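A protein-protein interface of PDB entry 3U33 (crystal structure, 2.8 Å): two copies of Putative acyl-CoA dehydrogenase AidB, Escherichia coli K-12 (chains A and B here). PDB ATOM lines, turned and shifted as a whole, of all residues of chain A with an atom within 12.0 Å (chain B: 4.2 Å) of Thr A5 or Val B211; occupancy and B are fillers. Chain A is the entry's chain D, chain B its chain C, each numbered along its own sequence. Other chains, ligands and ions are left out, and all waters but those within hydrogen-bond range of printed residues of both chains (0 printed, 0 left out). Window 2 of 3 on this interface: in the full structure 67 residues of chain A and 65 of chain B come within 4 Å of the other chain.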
ATOM      1  N   HIS A   2       8.644  12.252  -1.695  1.00  0.00           N
ATOM      2  CA  HIS A   2       7.356  12.937  -1.775  1.00  0.00           C
ATOM      3  C   HIS A   2       7.316  14.200  -0.909  1.00  0.00           C
ATOM      4  O   HIS A   2       6.356  14.972  -0.964  1.00  0.00           O
ATOM      5  CB  HIS A   2       6.206  11.987  -1.403  1.00  0.00           C
ATOM      6  CG  HIS A   2       6.012  11.804   0.073  1.00  0.00           C
ATOM      7  ND1 HIS A   2       5.389  12.745   0.866  1.00  0.00           N
ATOM      8  CD2 HIS A   2       6.341  10.779   0.896  1.00  0.00           C
ATOM      9  CE1 HIS A   2       5.350  12.313   2.113  1.00  0.00           C
ATOM     10  NE2 HIS A   2       5.921  11.123   2.159  1.00  0.00           N
ATOM     11  N   TRP A   3       8.366  14.404  -0.116  1.00  0.00           N
ATOM     12  CA  TRP A   3       8.461  15.580   0.751  1.00  0.00           C
ATOM     13  C   TRP A   3       8.823  16.841  -0.036  1.00  0.00           C
ATOM     14  O   TRP A   3       8.500  17.960   0.373  1.00  0.00           O
ATOM     15  CB  TRP A   3       9.497  15.355   1.860  1.00  0.00           C
ATOM     16  CG  TRP A   3       9.202  14.175   2.753  1.00  0.00           C
ATOM     17  CD1 TRP A   3       9.783  12.936   2.700  1.00  0.00           C
ATOM     18  CD2 TRP A   3       8.256  14.128   3.832  1.00  0.00           C
ATOM     19  NE1 TRP A   3       9.256  12.125   3.674  1.00  0.00           N
ATOM     20  CE2 TRP A   3       8.318  12.830   4.384  1.00  0.00           C
ATOM     21  CE3 TRP A   3       7.361  15.056   4.380  1.00  0.00           C
ATOM     22  CZ2 TRP A   3       7.517  12.438   5.457  1.00  0.00           C
ATOM     23  CZ3 TRP A   3       6.570  14.666   5.445  1.00  0.00           C
ATOM     24  CH2 TRP A   3       6.652  13.366   5.972  1.00  0.00           C
ATOM     25  N   GLN A   4       9.494  16.645  -1.167  1.00  0.00           N
ATOM     26  CA  GLN A   4       9.972  17.752  -1.986  1.00  0.00           C
ATOM     27  C   GLN A   4       8.885  18.317  -2.893  1.00  0.00           C
ATOM     28  O   GLN A   4       7.964  17.608  -3.292  1.00  0.00           O
ATOM     29  CB  GLN A   4      11.177  17.312  -2.823  1.00  0.00           C
ATOM     30  CG  GLN A   4      12.435  17.046  -2.008  1.00  0.00           C
ATOM     31  CD  GLN A   4      13.591  16.578  -2.873  1.00  0.00           C
ATOM     32  OE1 GLN A   4      13.423  16.334  -4.070  1.00  0.00           O
ATOM     33  NE2 GLN A   4      14.770  16.452  -2.273  1.00  0.00           N
ATOM     34  N   THR A   5       9.012  19.600  -3.215  1.00  0.00           N
ATOM     35  CA  THR A   5       8.070  20.276  -4.092  1.00  0.00           C
ATOM     36  C   THR A   5       8.688  20.491  -5.468  1.00  0.00           C
ATOM     37  O   THR A   5       7.993  20.837  -6.424  1.00  0.00           O
ATOM     38  CB  THR A   5       7.649  21.644  -3.511  1.00  0.00           C
ATOM     39  OG1 THR A   5       8.816  22.412  -3.187  1.00  0.00           O
ATOM     40  CG2 THR A   5       6.823  21.455  -2.249  1.00  0.00           C
ATOM     41  N   HIS A   6       9.998  20.281  -5.561  1.00  0.00           N
ATOM     42  CA  HIS A   6      10.729  20.529  -6.799  1.00  0.00           C
ATOM     43  C   HIS A   6      12.162  19.981  -6.739  1.00  0.00           C
ATOM     44  O   HIS A   6      12.653  19.608  -5.672  1.00  0.00           O
ATOM     45  CB  HIS A   6      10.778  22.031  -7.063  1.00  0.00           C
ATOM     46  CG  HIS A   6      11.653  22.779  -6.105  1.00  0.00           C
ATOM     47  ND1 HIS A   6      11.286  23.024  -4.798  1.00  0.00           N
ATOM     48  CD2 HIS A   6      12.882  23.327  -6.260  1.00  0.00           C
ATOM     49  CE1 HIS A   6      12.248  23.698  -4.191  1.00  0.00           C
ATOM     50  NE2 HIS A   6      13.228  23.896  -5.057  1.00  0.00           N
ATOM     51  N   THR A   7      12.827  19.940  -7.890  1.00  0.00           N
ATOM     52  CA  THR A   7      14.236  19.566  -7.941  1.00  0.00           C
ATOM     53  C   THR A   7      15.086  20.767  -8.343  1.00  0.00           C
ATOM     54  O   THR A   7      14.742  21.498  -9.278  1.00  0.00           O
ATOM     55  CB  THR A   7      14.484  18.417  -8.936  1.00  0.00           C
ATOM     56  OG1 THR A   7      13.639  17.306  -8.606  1.00  0.00           O
ATOM     57  CG2 THR A   7      15.945  17.978  -8.896  1.00  0.00           C
ATOM     58  N   VAL A   8      16.189  20.974  -7.627  1.00  0.00           N
ATOM     59  CA  VAL A   8      17.094  22.080  -7.928  1.00  0.00           C
ATOM     60  C   VAL A   8      18.071  21.663  -9.019  1.00  0.00           C
ATOM     61  O   VAL A   8      18.728  20.625  -8.906  1.00  0.00           O
ATOM     62  CB  VAL A   8      17.893  22.534  -6.682  1.00  0.00           C
ATOM     63  CG1 VAL A   8      18.883  23.618  -7.058  1.00  0.00           C
ATOM     64  CG2 VAL A   8      16.957  23.026  -5.590  1.00  0.00           C
ATOM     65  N   PHE A   9      18.157  22.467 -10.075  1.00  0.00           N
ATOM     66  CA  PHE A   9      19.075  22.191 -11.177  1.00  0.00           C
ATOM     67  C   PHE A   9      19.452  23.478 -11.906  1.00  0.00           C
ATOM     68  O   PHE A   9      18.819  24.520 -11.707  1.00  0.00           O
ATOM     69  CB  PHE A   9      18.469  21.174 -12.160  1.00  0.00           C
ATOM     70  CG  PHE A   9      17.280  21.698 -12.926  1.00  0.00           C
ATOM     71  CD1 PHE A   9      17.443  22.256 -14.190  1.00  0.00           C
ATOM     72  CD2 PHE A   9      16.003  21.642 -12.382  1.00  0.00           C
ATOM     73  CE1 PHE A   9      16.354  22.741 -14.899  1.00  0.00           C
ATOM     74  CE2 PHE A   9      14.907  22.129 -13.084  1.00  0.00           C
ATOM     75  CZ  PHE A   9      15.085  22.678 -14.345  1.00  0.00           C
ATOM     76  N   THR B 198       7.249  24.487 -11.877  1.00  0.00           N
ATOM     77  CA  THR B 198       6.076  24.565 -11.022  1.00  0.00           C
ATOM     78  C   THR B 198       4.886  24.083 -11.831  1.00  0.00           C
ATOM     79  O   THR B 198       4.553  24.671 -12.859  1.00  0.00           O
ATOM     80  CB  THR B 198       5.822  26.010 -10.544  1.00  0.00           C
ATOM     81  OG1 THR B 198       6.949  26.469  -9.787  1.00  0.00           O
ATOM     82  CG2 THR B 198       4.570  26.076  -9.679  1.00  0.00           C
ATOM     83  N   ARG B 199       4.258  23.003 -11.381  1.00  0.00           N
ATOM     84  CA  ARG B 199       3.171  22.397 -12.140  1.00  0.00           C
ATOM     85  C   ARG B 199       1.808  22.652 -11.504  1.00  0.00           C
ATOM     86  O   ARG B 199       1.686  22.755 -10.285  1.00  0.00           O
ATOM     87  CB  ARG B 199       3.408  20.892 -12.336  1.00  0.00           C
ATOM     88  N   ARG B 209      -4.305  22.867  -8.533  1.00  0.00           N
ATOM     89  CA  ARG B 209      -3.365  22.593  -7.457  1.00  0.00           C
ATOM     90  C   ARG B 209      -1.975  22.947  -7.961  1.00  0.00           C
ATOM     91  O   ARG B 209      -1.542  22.459  -9.003  1.00  0.00           O
ATOM     92  CB  ARG B 209      -3.415  21.120  -7.037  1.00  0.00           C
ATOM     93  N   LEU B 210      -1.282  23.813  -7.234  1.00  0.00           N
ATOM     94  CA  LEU B 210       0.079  24.168  -7.601  1.00  0.00           C
ATOM     95  C   LEU B 210       1.084  23.520  -6.667  1.00  0.00           C
ATOM     96  O   LEU B 210       0.928  23.551  -5.443  1.00  0.00           O
ATOM     97  CB  LEU B 210       0.274  25.682  -7.633  1.00  0.00           C
ATOM     98  CG  LEU B 210      -0.133  26.349  -8.947  1.00  0.00           C
ATOM     99  CD1 LEU B 210      -1.652  26.334  -9.129  1.00  0.00           C
ATOM    100  CD2 LEU B 210       0.406  27.766  -9.003  1.00  0.00           C
ATOM    101  N   VAL B 211       2.101  22.911  -7.265  1.00  0.00           N
ATOM    102  CA  VAL B 211       3.216  22.341  -6.532  1.00  0.00           C
ATOM    103  C   VAL B 211       4.494  22.797  -7.225  1.00  0.00           C
ATOM    104  O   VAL B 211       4.661  22.610  -8.429  1.00  0.00           O
ATOM    105  CB  VAL B 211       3.169  20.796  -6.521  1.00  0.00           C
ATOM    106  CG1 VAL B 211       4.357  20.236  -5.746  1.00  0.00           C
ATOM    107  CG2 VAL B 211       1.860  20.301  -5.923  1.00  0.00           C
ATOM    108  N   GLY B 212       5.390  23.409  -6.464  1.00  0.00           N
ATOM    109  CA  GLY B 212       6.626  23.925  -7.022  1.00  0.00           C
ATOM    110  C   GLY B 212       7.300  24.907  -6.082  1.00  0.00           C
ATOM    111  O   GLY B 212       7.202  24.785  -4.853  1.00  0.00           O
ATOM    112  N   GLU B 272       7.753  27.950  -1.454  1.00  0.00           N
ATOM    113  CA  GLU B 272       7.411  26.678  -2.070  1.00  0.00           C
ATOM    114  C   GLU B 272       5.902  26.487  -1.998  1.00  0.00           C
ATOM    115  O   GLU B 272       5.277  26.872  -1.013  1.00  0.00           O
ATOM    116  CB  GLU B 272       8.145  25.521  -1.385  1.00  0.00           C
ATOM    117  CG  GLU B 272       9.664  25.560  -1.534  1.00  0.00           C
ATOM    118  CD  GLU B 272      10.357  24.407  -0.818  1.00  0.00           C
ATOM    119  OE1 GLU B 272       9.655  23.460  -0.392  1.00  0.00           O
ATOM    120  OE2 GLU B 272      11.604  24.456  -0.678  1.00  0.00           O
ATOM    121  N   PHE B 273       5.326  25.920  -3.057  1.00  0.00           N
ATOM    122  CA  PHE B 273       3.891  25.660  -3.109  1.00  0.00           C
ATOM    123  C   PHE B 273       3.612  24.214  -2.758  1.00  0.00           C
ATOM    124  O   PHE B 273       4.108  23.298  -3.422  1.00  0.00           O
ATOM    125  CB  PHE B 273       3.332  25.967  -4.494  1.00  0.00           C
ATOM    126  CG  PHE B 273       3.629  27.354  -4.965  1.00  0.00           C
ATOM    127  CD1 PHE B 273       3.105  28.448  -4.299  1.00  0.00           C
ATOM    128  CD2 PHE B 273       4.434  27.564  -6.071  1.00  0.00           C
ATOM    129  CE1 PHE B 273       3.377  29.728  -4.721  1.00  0.00           C
ATOM    130  CE2 PHE B 273       4.715  28.845  -6.500  1.00  0.00           C
ATOM    131  CZ  PHE B 273       4.181  29.931  -5.823  1.00  0.00           C
ATOM    132  N   GLN B 274       2.824  24.014  -1.706  1.00  0.00           N
ATOM    133  CA  GLN B 274       2.439  22.677  -1.282  1.00  0.00           C
ATOM    134  C   GLN B 274       0.952  22.442  -1.534  1.00  0.00           C
ATOM    135  O   GLN B 274       0.131  22.478  -0.612  1.00  0.00           O
ATOM    136  CB  GLN B 274       2.795  22.459   0.184  1.00  0.00           C
ATOM    137  CG  GLN B 274       4.290  22.419   0.415  1.00  0.00           C
ATOM    138  CD  GLN B 274       4.648  22.187   1.861  1.00  0.00           C
ATOM    139  OE1 GLN B 274       3.814  22.343   2.749  1.00  0.00           O
ATOM    140  NE2 GLN B 274       5.899  21.812   2.107  1.00  0.00           N
ATOM    141  N   ASP B 275       0.628  22.200  -2.802  1.00  0.00           N
ATOM    142  CA  ASP B 275      -0.748  22.027  -3.236  1.00  0.00           C
ATOM    143  C   ASP B 275      -1.531  23.293  -2.945  1.00  0.00           C
ATOM    144  O   ASP B 275      -2.636  23.247  -2.395  1.00  0.00           O
ATOM    145  CB  ASP B 275      -1.391  20.801  -2.570  1.00  0.00           C
ATOM    146  CG  ASP B 275      -0.911  19.483  -3.182  1.00  0.00           C
ATOM    147  OD1 ASP B 275      -0.835  19.395  -4.430  1.00  0.00           O
ATOM    148  OD2 ASP B 275      -0.604  18.539  -2.419  1.00  0.00           O
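O of Gly B212 lies within hydrogen-bond range of OG1 of Thr A5.
The side-chain hydroxyl of Thr A5 sits at hydrogen-bond distance from the side-chain carboxylate of Glu B272.
OG1 of Thr A5 is in hydrogen-bond range of ND1 of His A6.
The backbone NH (N) of Arg B199 lies within hydrogen-bond range of the backbone carbonyl oxygen (O) of Val B211 (3.0 Å).
N of Phe B273 sits at hydrogen-bond distance from O of Gly B212 (2.8 Å).
CG1 of Val B211 touches O of Thr A5, at 3.7 Å.
Thr A5 touches Phe B273.
Thr A5 touches Gln B274 (CG2 to CG, 3.8 Å).
Glu B272 touches His A6.
Trp A3 touches none of the printed residues of chain B.
Of chain B, only Val B211 (3.7 Å), Gly B212 (3.3 Å), Glu B272 (3.1 Å), Phe B273 (3.5 Å) and Gln B274 (3.8 Å) come within 4 Å of Thr A5.
Of the printed residues of chain B, His A6 touches Glu B272 (3.7 Å).
Thr B198 touches none of the printed residues of chain A.
No residue of chain A comes within 4 Å of Arg B199.
No residue of chain A comes within 4 Å of Leu B210.
Val B211 touches just one residue of chain A: Thr A5.
Of the printed residues of chain A, Glu B272 touches Thr A5 and His A6.
Gln B274 touches just one residue of chain A: Thr A5.
Asp B275 touches none of the printed residues of chain A.
The nearest printed residue of chain B that does not touch His A6 is Gly B212 (4.4 Å).
Of the 8 printed residues of chain A, 2 touch a printed residue of chain B.
Printed residues of chain A that touch a printed residue of chain B: Thr A5 and His A6.
Hydrophobic or aromatic side chains of chain A within 4 Å of the printed part of chain B: His A6.
Along chain A the printed residues that touch a printed residue of chain B span positions 5 to 6.
Printed residues of chain B that touch a printed residue of chain A: Val B211, Gly B212, Glu B272, Phe B273 and Gln B274.
Among the printed residues, 6 pairs touch across the chains.
Among the printed residues, no Asp or Glu carboxylate lies within 4 Å of a Lys or Arg side-chain nitrogen of the other chain.
No position is printed for both chains.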
